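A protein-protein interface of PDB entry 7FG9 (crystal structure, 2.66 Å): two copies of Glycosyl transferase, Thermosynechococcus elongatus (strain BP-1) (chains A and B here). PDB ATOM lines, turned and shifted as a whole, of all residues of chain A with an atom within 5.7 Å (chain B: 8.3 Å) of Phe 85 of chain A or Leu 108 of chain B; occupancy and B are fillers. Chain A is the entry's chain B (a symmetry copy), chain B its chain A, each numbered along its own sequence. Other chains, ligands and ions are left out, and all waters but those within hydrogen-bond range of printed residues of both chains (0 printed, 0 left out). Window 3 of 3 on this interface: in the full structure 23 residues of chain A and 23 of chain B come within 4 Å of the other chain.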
ATOM      1  N   GLN A  80       6.327  -8.369  23.590  1.00  0.00           N
ATOM      2  CA  GLN A  80       7.344  -7.782  24.456  1.00  0.00           C
ATOM      3  C   GLN A  80       8.029  -6.595  23.790  1.00  0.00           C
ATOM      4  O   GLN A  80       8.199  -5.541  24.410  1.00  0.00           O
ATOM      5  CB  GLN A  80       8.360  -8.854  24.836  1.00  0.00           C
ATOM      6  CG  GLN A  80       9.486  -8.378  25.717  1.00  0.00           C
ATOM      7  CD  GLN A  80      10.631  -9.395  25.795  1.00  0.00           C
ATOM      8  OE1 GLN A  80      11.085  -9.946  24.770  1.00  0.00           O
ATOM      9  NE2 GLN A  80      11.078  -9.671  27.021  1.00  0.00           N
ATOM     10  N   LEU A  81       8.451  -6.745  22.533  1.00  0.00           N
ATOM     11  CA  LEU A  81       8.939  -5.586  21.793  1.00  0.00           C
ATOM     12  C   LEU A  81       7.904  -4.461  21.816  1.00  0.00           C
ATOM     13  O   LEU A  81       8.252  -3.276  21.922  1.00  0.00           O
ATOM     14  CB  LEU A  81       9.273  -5.985  20.351  1.00  0.00           C
ATOM     15  CG  LEU A  81      10.486  -6.888  20.183  1.00  0.00           C
ATOM     16  CD1 LEU A  81      10.555  -7.409  18.775  1.00  0.00           C
ATOM     17  CD2 LEU A  81      11.744  -6.136  20.528  1.00  0.00           C
ATOM     18  N   GLY A  82       6.620  -4.826  21.719  1.00  0.00           N
ATOM     19  CA  GLY A  82       5.572  -3.834  21.835  1.00  0.00           C
ATOM     20  C   GLY A  82       5.584  -3.148  23.184  1.00  0.00           C
ATOM     21  O   GLY A  82       5.616  -1.921  23.272  1.00  0.00           O
ATOM     22  N   GLU A  83       5.577  -3.930  24.259  1.00  0.00           N
ATOM     23  CA  GLU A  83       5.526  -3.296  25.571  1.00  0.00           C
ATOM     24  C   GLU A  83       6.785  -2.484  25.842  1.00  0.00           C
ATOM     25  O   GLU A  83       6.720  -1.471  26.537  1.00  0.00           O
ATOM     26  CB  GLU A  83       5.260  -4.336  26.669  1.00  0.00           C
ATOM     27  CG  GLU A  83       3.777  -4.862  26.726  1.00  0.00           C
ATOM     28  CD  GLU A  83       2.685  -3.738  26.948  1.00  0.00           C
ATOM     29  OE1 GLU A  83       2.076  -3.667  28.054  1.00  0.00           O
ATOM     30  OE2 GLU A  83       2.387  -2.970  25.983  1.00  0.00           O
ATOM     31  N   VAL A  84       7.918  -2.871  25.253  1.00  0.00           N
ATOM     32  CA  VAL A  84       9.165  -2.143  25.474  1.00  0.00           C
ATOM     33  C   VAL A  84       9.150  -0.804  24.741  1.00  0.00           C
ATOM     34  O   VAL A  84       9.226   0.262  25.365  1.00  0.00           O
ATOM     35  CB  VAL A  84      10.373  -2.993  25.052  1.00  0.00           C
ATOM     36  CG1 VAL A  84      11.622  -2.163  25.098  1.00  0.00           C
ATOM     37  CG2 VAL A  84      10.524  -4.148  25.980  1.00  0.00           C
ATOM     38  N   PHE A  85       9.059  -0.832  23.409  1.00  0.00           N
ATOM     39  CA  PHE A  85       9.247   0.391  22.635  1.00  0.00           C
ATOM     40  C   PHE A  85       8.039   1.324  22.656  1.00  0.00           C
ATOM     41  O   PHE A  85       8.215   2.528  22.457  1.00  0.00           O
ATOM     42  CB  PHE A  85       9.650   0.042  21.207  1.00  0.00           C
ATOM     43  CG  PHE A  85      11.041  -0.492  21.121  1.00  0.00           C
ATOM     44  CD1 PHE A  85      11.271  -1.861  21.021  1.00  0.00           C
ATOM     45  CD2 PHE A  85      12.128   0.363  21.223  1.00  0.00           C
ATOM     46  CE1 PHE A  85      12.558  -2.361  20.980  1.00  0.00           C
ATOM     47  CE2 PHE A  85      13.420  -0.130  21.184  1.00  0.00           C
ATOM     48  CZ  PHE A  85      13.640  -1.490  21.059  1.00  0.00           C
ATOM     49  N   SER A  86       6.833   0.830  22.947  1.00  0.00           N
ATOM     50  CA  SER A  86       5.764   1.777  23.264  1.00  0.00           C
ATOM     51  C   SER A  86       6.013   2.529  24.575  1.00  0.00           C
ATOM     52  O   SER A  86       5.233   3.424  24.916  1.00  0.00           O
ATOM     53  CB  SER A  86       4.402   1.073  23.327  1.00  0.00           C
ATOM     54  OG  SER A  86       4.143   0.510  24.607  1.00  0.00           O
ATOM     55  N   ARG A  87       7.067   2.196  25.316  1.00  0.00           N
ATOM     56  CA  ARG A  87       7.404   2.873  26.561  1.00  0.00           C
ATOM     57  C   ARG A  87       8.786   3.505  26.483  1.00  0.00           C
ATOM     58  O   ARG A  87       9.448   3.676  27.507  1.00  0.00           O
ATOM     59  CB  ARG A  87       7.337   1.902  27.738  1.00  0.00           C
ATOM     60  CG  ARG A  87       5.946   1.443  28.071  1.00  0.00           C
ATOM     61  CD  ARG A  87       5.898   0.718  29.405  1.00  0.00           C
ATOM     62  NE  ARG A  87       4.938  -0.378  29.342  1.00  0.00           N
ATOM     63  CZ  ARG A  87       4.217  -0.806  30.372  1.00  0.00           C
ATOM     64  NH1 ARG A  87       4.356  -0.231  31.568  1.00  0.00           N
ATOM     65  NH2 ARG A  87       3.353  -1.802  30.196  1.00  0.00           N
ATOM     66  N   ALA A  88       9.236   3.849  25.268  1.00  0.00           N
ATOM     67  CA  ALA A  88      10.590   4.376  25.087  1.00  0.00           C
ATOM     68  C   ALA A  88      10.881   5.562  26.007  1.00  0.00           C
ATOM     69  O   ALA A  88      11.956   5.638  26.612  1.00  0.00           O
ATOM     70  CB  ALA A  88      10.809   4.770  23.627  1.00  0.00           C
ATOM     71  N   ASN A  89       9.931   6.485  26.147  1.00  0.00           N
ATOM     72  CA  ASN A  89      10.198   7.712  26.887  1.00  0.00           C
ATOM     73  C   ASN A  89      10.262   7.504  28.396  1.00  0.00           C
ATOM     74  O   ASN A  89      10.437   8.487  29.128  1.00  0.00           O
ATOM     75  CB  ASN A  89       9.136   8.761  26.552  1.00  0.00           C
ATOM     76  CG  ASN A  89       9.306   9.342  25.141  1.00  0.00           C
ATOM     77  OD1 ASN A  89       9.753   8.652  24.211  1.00  0.00           O
ATOM     78  ND2 ASN A  89       8.946  10.621  24.980  1.00  0.00           N
ATOM     79  N   ILE A  94      17.846   1.633  26.938  1.00  0.00           N
ATOM     80  CA  ILE A  94      17.147   0.365  26.792  1.00  0.00           C
ATOM     81  C   ILE A  94      18.201  -0.691  26.530  1.00  0.00           C
ATOM     82  O   ILE A  94      18.958  -0.584  25.555  1.00  0.00           O
ATOM     83  CB  ILE A  94      16.121   0.409  25.646  1.00  0.00           C
ATOM     84  CG1 ILE A  94      14.948   1.319  25.996  1.00  0.00           C
ATOM     85  CG2 ILE A  94      15.647  -1.009  25.259  1.00  0.00           C
ATOM     86  CD1 ILE A  94      14.046   1.630  24.847  1.00  0.00           C
ATOM     87  N   ALA A 102      15.210  -6.560  17.621  1.00  0.00           N
ATOM     88  CA  ALA A 102      15.107  -5.250  18.234  1.00  0.00           C
ATOM     89  C   ALA A 102      15.706  -4.149  17.368  1.00  0.00           C
ATOM     90  O   ALA A 102      15.460  -2.970  17.644  1.00  0.00           O
ATOM     91  CB  ALA A 102      15.781  -5.261  19.600  1.00  0.00           C
ATOM     92  N   TYR A 105      12.996  -1.536  15.406  1.00  0.00           N
ATOM     93  CA  TYR A 105      12.356  -0.673  16.396  1.00  0.00           C
ATOM     94  C   TYR A 105      13.258   0.485  16.782  1.00  0.00           C
ATOM     95  O   TYR A 105      12.791   1.617  16.968  1.00  0.00           O
ATOM     96  CB  TYR A 105      11.984  -1.479  17.644  1.00  0.00           C
ATOM     97  CG  TYR A 105      10.880  -2.480  17.405  1.00  0.00           C
ATOM     98  CD1 TYR A 105       9.547  -2.131  17.592  1.00  0.00           C
ATOM     99  CD2 TYR A 105      11.170  -3.775  16.969  1.00  0.00           C
ATOM    100  CE1 TYR A 105       8.534  -3.047  17.370  1.00  0.00           C
ATOM    101  CE2 TYR A 105      10.164  -4.696  16.734  1.00  0.00           C
ATOM    102  CZ  TYR A 105       8.851  -4.327  16.941  1.00  0.00           C
ATOM    103  OH  TYR A 105       7.842  -5.237  16.710  1.00  0.00           O
ATOM    104  N   THR A 106      14.557   0.222  16.892  1.00  0.00           N
ATOM    105  CA  THR A 106      15.476   1.197  17.472  1.00  0.00           C
ATOM    106  C   THR A 106      15.552   2.466  16.622  1.00  0.00           C
ATOM    107  O   THR A 106      15.632   3.582  17.157  1.00  0.00           O
ATOM    108  CB  THR A 106      16.857   0.551  17.628  1.00  0.00           C
ATOM    109  OG1 THR A 106      16.735  -0.677  18.362  1.00  0.00           O
ATOM    110  CG2 THR A 106      17.801   1.481  18.387  1.00  0.00           C
ATOM    111  N   LEU A 108      13.179   3.844  15.279  1.00  0.00           N
ATOM    112  CA  LEU A 108      11.861   4.448  15.284  1.00  0.00           C
ATOM    113  C   LEU A 108      11.536   5.176  16.577  1.00  0.00           C
ATOM    114  O   LEU A 108      10.505   5.861  16.645  1.00  0.00           O
ATOM    115  CB  LEU A 108      10.791   3.377  15.038  1.00  0.00           C
ATOM    116  CG  LEU A 108      10.690   2.858  13.611  1.00  0.00           C
ATOM    117  CD1 LEU A 108       9.941   1.521  13.596  1.00  0.00           C
ATOM    118  CD2 LEU A 108       9.979   3.895  12.763  1.00  0.00           C
ATOM    119  N   VAL A 109      12.354   5.020  17.609  1.00  0.00           N
ATOM    120  CA  VAL A 109      12.211   5.765  18.846  1.00  0.00           C
ATOM    121  C   VAL A 109      13.480   6.575  19.028  1.00  0.00           C
ATOM    122  O   VAL A 109      14.477   6.379  18.329  1.00  0.00           O
ATOM    123  CB  VAL A 109      11.963   4.861  20.062  1.00  0.00           C
ATOM    124  CG1 VAL A 109      10.644   4.111  19.894  1.00  0.00           C
ATOM    125  CG2 VAL A 109      13.136   3.918  20.264  1.00  0.00           C
ATOM    126  N   VAL A 113      19.560   2.638  22.623  1.00  0.00           N
ATOM    127  CA  VAL A 113      19.428   1.211  22.902  1.00  0.00           C
ATOM    128  C   VAL A 113      20.814   0.565  22.846  1.00  0.00           C
ATOM    129  O   VAL A 113      21.631   0.877  21.968  1.00  0.00           O
ATOM    130  CB  VAL A 113      18.447   0.534  21.905  1.00  0.00           C
ATOM    131  CG1 VAL A 113      18.411  -1.005  22.069  1.00  0.00           C
ATOM    132  CG2 VAL A 113      17.055   1.109  22.048  1.00  0.00           C
ATOM    133  N   PHE B  85       8.169   0.710   7.751  1.00  0.00           N
ATOM    134  CA  PHE B  85       7.724   1.647   8.771  1.00  0.00           C
ATOM    135  C   PHE B  85       8.690   2.807   8.983  1.00  0.00           C
ATOM    136  O   PHE B  85       8.272   3.849   9.493  1.00  0.00           O
ATOM    137  CB  PHE B  85       7.476   0.890  10.077  1.00  0.00           C
ATOM    138  CG  PHE B  85       6.210   0.099  10.058  1.00  0.00           C
ATOM    139  CD1 PHE B  85       6.217  -1.241   9.701  1.00  0.00           C
ATOM    140  CD2 PHE B  85       4.994   0.706  10.344  1.00  0.00           C
ATOM    141  CE1 PHE B  85       5.030  -1.969   9.659  1.00  0.00           C
ATOM    142  CE2 PHE B  85       3.808  -0.019  10.301  1.00  0.00           C
ATOM    143  CZ  PHE B  85       3.832  -1.359   9.958  1.00  0.00           C
ATOM    144  N   ALA B  88       7.215   5.308   6.766  1.00  0.00           N
ATOM    145  CA  ALA B  88       5.764   5.326   6.949  1.00  0.00           C
ATOM    146  C   ALA B  88       5.114   6.575   6.363  1.00  0.00           C
ATOM    147  O   ALA B  88       3.983   6.505   5.869  1.00  0.00           O
ATOM    148  CB  ALA B  88       5.402   5.198   8.433  1.00  0.00           C
ATOM    149  N   ASN B  89       5.793   7.717   6.391  1.00  0.00           N
ATOM    150  CA  ASN B  89       5.133   8.940   5.957  1.00  0.00           C
ATOM    151  C   ASN B  89       5.277   9.205   4.459  1.00  0.00           C
ATOM    152  O   ASN B  89       4.832  10.254   3.983  1.00  0.00           O
ATOM    153  CB  ASN B  89       5.612  10.128   6.793  1.00  0.00           C
ATOM    154  CG  ASN B  89       4.637  10.439   7.945  1.00  0.00           C
ATOM    155  OD1 ASN B  89       3.448  10.717   7.710  1.00  0.00           O
ATOM    156  ND2 ASN B  89       5.125  10.351   9.190  1.00  0.00           N
ATOM    157  N   ALA B 102       3.516  -7.140  12.503  1.00  0.00           N
ATOM    158  CA  ALA B 102       3.372  -5.720  12.222  1.00  0.00           C
ATOM    159  C   ALA B 102       2.521  -4.991  13.250  1.00  0.00           C
ATOM    160  O   ALA B 102       2.497  -3.756  13.235  1.00  0.00           O
ATOM    161  CB  ALA B 102       2.767  -5.506  10.832  1.00  0.00           C
ATOM    162  N   LEU B 103       1.819  -5.708  14.130  1.00  0.00           N
ATOM    163  CA  LEU B 103       0.939  -5.037  15.088  1.00  0.00           C
ATOM    164  C   LEU B 103       1.679  -4.044  15.976  1.00  0.00           C
ATOM    165  O   LEU B 103       1.266  -2.870  16.019  1.00  0.00           O
ATOM    166  CB  LEU B 103       0.173  -6.071  15.927  1.00  0.00           C
ATOM    167  CG  LEU B 103      -0.818  -6.970  15.185  1.00  0.00           C
ATOM    168  CD1 LEU B 103      -1.405  -8.006  16.130  1.00  0.00           C
ATOM    169  CD2 LEU B 103      -1.903  -6.143  14.530  1.00  0.00           C
ATOM    170  N   PRO B 104       2.767  -4.407  16.680  1.00  0.00           N
ATOM    171  CA  PRO B 104       3.433  -3.399  17.527  1.00  0.00           C
ATOM    172  C   PRO B 104       4.044  -2.246  16.750  1.00  0.00           C
ATOM    173  O   PRO B 104       4.038  -1.112  17.245  1.00  0.00           O
ATOM    174  CB  PRO B 104       4.498  -4.212  18.285  1.00  0.00           C
ATOM    175  CG  PRO B 104       4.692  -5.440  17.492  1.00  0.00           C
ATOM    176  CD  PRO B 104       3.387  -5.741  16.833  1.00  0.00           C
ATOM    177  N   TYR B 105       4.573  -2.485  15.551  1.00  0.00           N
ATOM    178  CA  TYR B 105       5.053  -1.370  14.728  1.00  0.00           C
ATOM    179  C   TYR B 105       3.970  -0.319  14.510  1.00  0.00           C
ATOM    180  O   TYR B 105       4.255   0.881  14.502  1.00  0.00           O
ATOM    181  CB  TYR B 105       5.544  -1.871  13.370  1.00  0.00           C
ATOM    182  CG  TYR B 105       6.869  -2.554  13.412  1.00  0.00           C
ATOM    183  CD1 TYR B 105       8.037  -1.839  13.182  1.00  0.00           C
ATOM    184  CD2 TYR B 105       6.965  -3.927  13.683  1.00  0.00           C
ATOM    185  CE1 TYR B 105       9.280  -2.465  13.211  1.00  0.00           C
ATOM    186  CE2 TYR B 105       8.208  -4.568  13.727  1.00  0.00           C
ATOM    187  CZ  TYR B 105       9.359  -3.818  13.490  1.00  0.00           C
ATOM    188  OH  TYR B 105      10.595  -4.408  13.512  1.00  0.00           O
ATOM    189  N   THR B 106       2.724  -0.756  14.315  1.00  0.00           N
ATOM    190  CA  THR B 106       1.637   0.171  14.008  1.00  0.00           C
ATOM    191  C   THR B 106       1.410   1.204  15.112  1.00  0.00           C
ATOM    192  O   THR B 106       0.991   2.337  14.825  1.00  0.00           O
ATOM    193  CB  THR B 106       0.367  -0.631  13.709  1.00  0.00           C
ATOM    194  OG1 THR B 106       0.631  -1.544  12.630  1.00  0.00           O
ATOM    195  CG2 THR B 106      -0.794   0.264  13.351  1.00  0.00           C
ATOM    196  N   SER B 107       1.708   0.852  16.364  1.00  0.00           N
ATOM    197  CA  SER B 107       1.638   1.809  17.466  1.00  0.00           C
ATOM    198  C   SER B 107       2.741   2.866  17.422  1.00  0.00           C
ATOM    199  O   SER B 107       2.598   3.907  18.066  1.00  0.00           O
ATOM    200  CB  SER B 107       1.707   1.061  18.792  1.00  0.00           C
ATOM    201  OG  SER B 107       0.759   0.016  18.802  1.00  0.00           O
ATOM    202  N   LEU B 108       3.828   2.639  16.686  1.00  0.00           N
ATOM    203  CA  LEU B 108       4.951   3.570  16.642  1.00  0.00           C
ATOM    204  C   LEU B 108       4.907   4.547  15.465  1.00  0.00           C
ATOM    205  O   LEU B 108       5.815   5.384  15.338  1.00  0.00           O
ATOM    206  CB  LEU B 108       6.288   2.804  16.609  1.00  0.00           C
ATOM    207  CG  LEU B 108       6.473   1.619  17.558  1.00  0.00           C
ATOM    208  CD1 LEU B 108       7.794   0.929  17.266  1.00  0.00           C
ATOM    209  CD2 LEU B 108       6.427   2.099  18.999  1.00  0.00           C
ATOM    210  N   VAL B 109       3.907   4.459  14.593  1.00  0.00           N
ATOM    211  CA  VAL B 109       3.808   5.389  13.481  1.00  0.00           C
ATOM    212  C   VAL B 109       2.407   5.968  13.484  1.00  0.00           C
ATOM    213  O   VAL B 109       1.457   5.332  13.952  1.00  0.00           O
ATOM    214  CB  VAL B 109       4.114   4.726  12.117  1.00  0.00           C
ATOM    215  CG1 VAL B 109       5.453   4.019  12.161  1.00  0.00           C
ATOM    216  CG2 VAL B 109       3.014   3.789  11.690  1.00  0.00           C
ATOM    217  N   LYS B 110       2.284   7.196  12.970  1.00  0.00           N
ATOM    218  CA  LYS B 110       0.969   7.817  12.848  1.00  0.00           C
ATOM    219  C   LYS B 110       0.209   7.282  11.641  1.00  0.00           C
ATOM    220  O   LYS B 110      -1.016   7.157  11.708  1.00  0.00           O
ATOM    221  CB  LYS B 110       1.076   9.350  12.754  1.00  0.00           C
ATOM    222  CG  LYS B 110       1.727  10.091  13.951  1.00  0.00           C
ATOM    223  CD  LYS B 110       0.998   9.883  15.296  1.00  0.00           C
ATOM    224  CE  LYS B 110       1.824   8.986  16.263  1.00  0.00           C
ATOM    225  NZ  LYS B 110       1.159   8.716  17.570  1.00  0.00           N
ATOM    226  N   THR B 111       0.916   6.945  10.550  1.00  0.00           N
ATOM    227  CA  THR B 111       0.256   6.498   9.324  1.00  0.00           C
ATOM    228  C   THR B 111      -0.639   5.287   9.588  1.00  0.00           C
ATOM    229  O   THR B 111      -0.184   4.299  10.170  1.00  0.00           O
ATOM    230  CB  THR B 111       1.282   6.143   8.256  1.00  0.00           C
ATOM    231  OG1 THR B 111       2.089   7.292   7.961  1.00  0.00           O
ATOM    232  CG2 THR B 111       0.569   5.675   6.992  1.00  0.00           C
ATOM    233  N   VAL B 113      -2.672   1.785   9.361  1.00  0.00           N
ATOM    234  CA  VAL B 113      -2.325   0.467   8.834  1.00  0.00           C
ATOM    235  C   VAL B 113      -3.593  -0.368   8.676  1.00  0.00           C
ATOM    236  O   VAL B 113      -4.501  -0.288   9.508  1.00  0.00           O
ATOM    237  CB  VAL B 113      -1.308  -0.240   9.754  1.00  0.00           C
ATOM    238  CG1 VAL B 113      -1.017  -1.673   9.275  1.00  0.00           C
ATOM    239  CG2 VAL B 113      -0.037   0.577   9.844  1.00  0.00           C
ATOM    240  N   TYR B 132      -4.073  -5.705  20.568  1.00  0.00           N
ATOM    241  CA  TYR B 132      -4.128  -4.698  19.519  1.00  0.00           C
ATOM    242  C   TYR B 132      -5.483  -4.743  18.826  1.00  0.00           C
ATOM    243  O   TYR B 132      -5.597  -4.534  17.615  1.00  0.00           O
ATOM    244  CB  TYR B 132      -2.980  -4.885  18.531  1.00  0.00           C
ATOM    245  CG  TYR B 132      -1.611  -4.644  19.137  1.00  0.00           C
ATOM    246  CD1 TYR B 132      -1.106  -3.349  19.271  1.00  0.00           C
ATOM    247  CD2 TYR B 132      -0.811  -5.707  19.565  1.00  0.00           C
ATOM    248  CE1 TYR B 132       0.153  -3.112  19.814  1.00  0.00           C
ATOM    249  CE2 TYR B 132       0.465  -5.484  20.117  1.00  0.00           C
ATOM    250  CZ  TYR B 132       0.940  -4.177  20.235  1.00  0.00           C
ATOM    251  OH  TYR B 132       2.197  -3.919  20.771  1.00  0.00           O
ATOM    252  N   GLN B 135      -7.104  -2.083  16.161  1.00  0.00           N
ATOM    253  CA  GLN B 135      -6.489  -1.769  14.882  1.00  0.00           C
ATOM    254  C   GLN B 135      -7.383  -2.235  13.736  1.00  0.00           C
ATOM    255  O   GLN B 135      -8.385  -2.922  13.929  1.00  0.00           O
ATOM    256  CB  GLN B 135      -5.106  -2.400  14.807  1.00  0.00           C
ATOM    257  CG  GLN B 135      -4.199  -1.858  15.873  1.00  0.00           C
ATOM    258  CD  GLN B 135      -2.748  -1.932  15.490  1.00  0.00           C
ATOM    259  OE1 GLN B 135      -2.361  -2.729  14.640  1.00  0.00           O
ATOM    260  NE2 GLN B 135      -1.933  -1.082  16.104  1.00  0.00           N
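Printed residues of chain B within 4 Å of Gly 82 of chain A: Pro 104 (3.7 Å) and Tyr 132 (3.5 Å). Glu 83 of chain A touches none of the printed residues of chain B. Val 84 of chain A touches none of the printed residues of chain B. Of the printed residues of chain B, Phe 85 of chain A touches Leu 108. Of the printed residues of chain A, Phe 85 of chain B touches Leu 108. Of the printed residues of chain A, Tyr 105 of chain B touches Tyr 105 and Leu 108. Leu 108 of chain B touches two residues of chain A. The nearest printed residue of chain B that does not touch Tyr 105 of chain A is Leu 103 of chain B (6.3 Å).
OG of Ser 86 of chain A sits at hydrogen-bond distance from O of Gly 82 of chain A (3.1 Å).
Among the printed residues, pairs that only touch across the chains: Tyr 105 of chain A with Tyr 105 of chain B (3.1 Å), Tyr 105 of chain A with Pro 104 of chain B (3.3 Å), Gly 82 of chain A with Tyr 132 of chain B (3.5 Å), Tyr 105 of chain A with Leu 108 of chain B (3.5 Å), Leu 108 of chain A with Phe 85 of chain B (3.7 Å), Gly 82 of chain A with Pro 104 of chain B (3.7 Å), Leu 108 of chain A with Tyr 105 of chain B (3.9 Å) and Phe 85 of chain A with Leu 108 of chain B (3.9 Å).
Phe 85 of chain A touches Leu 108 of chain B, and with the chains exchanged Leu 108 of chain A touches Phe 85 of chain B. Tyr 105 of chain A touches its own counterpart, Tyr 105 of chain B. Tyr 105 of chain A touches Leu 108 of chain B, and with the chains exchanged Leu 108 of chain A touches Tyr 105 of chain B. Positions printed for both chains: 85, 88, 89, 102, 105, 106, 108, 109 and 113. Of the 8 pairs that touch across the chains among the printed residues, 5 have their exchanged pair printed and touching as well.
Hydrophobic or aromatic side chains of chain A that line the printed part of chain B: Tyr 105 and Leu 108. Along chain A the printed residues that touch a printed residue of chain B span positions 82 to 108. Printed residues of chain B that touch a printed residue of chain A: Phe 85, Pro 104, Tyr 105, Leu 108 and Tyr 132.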
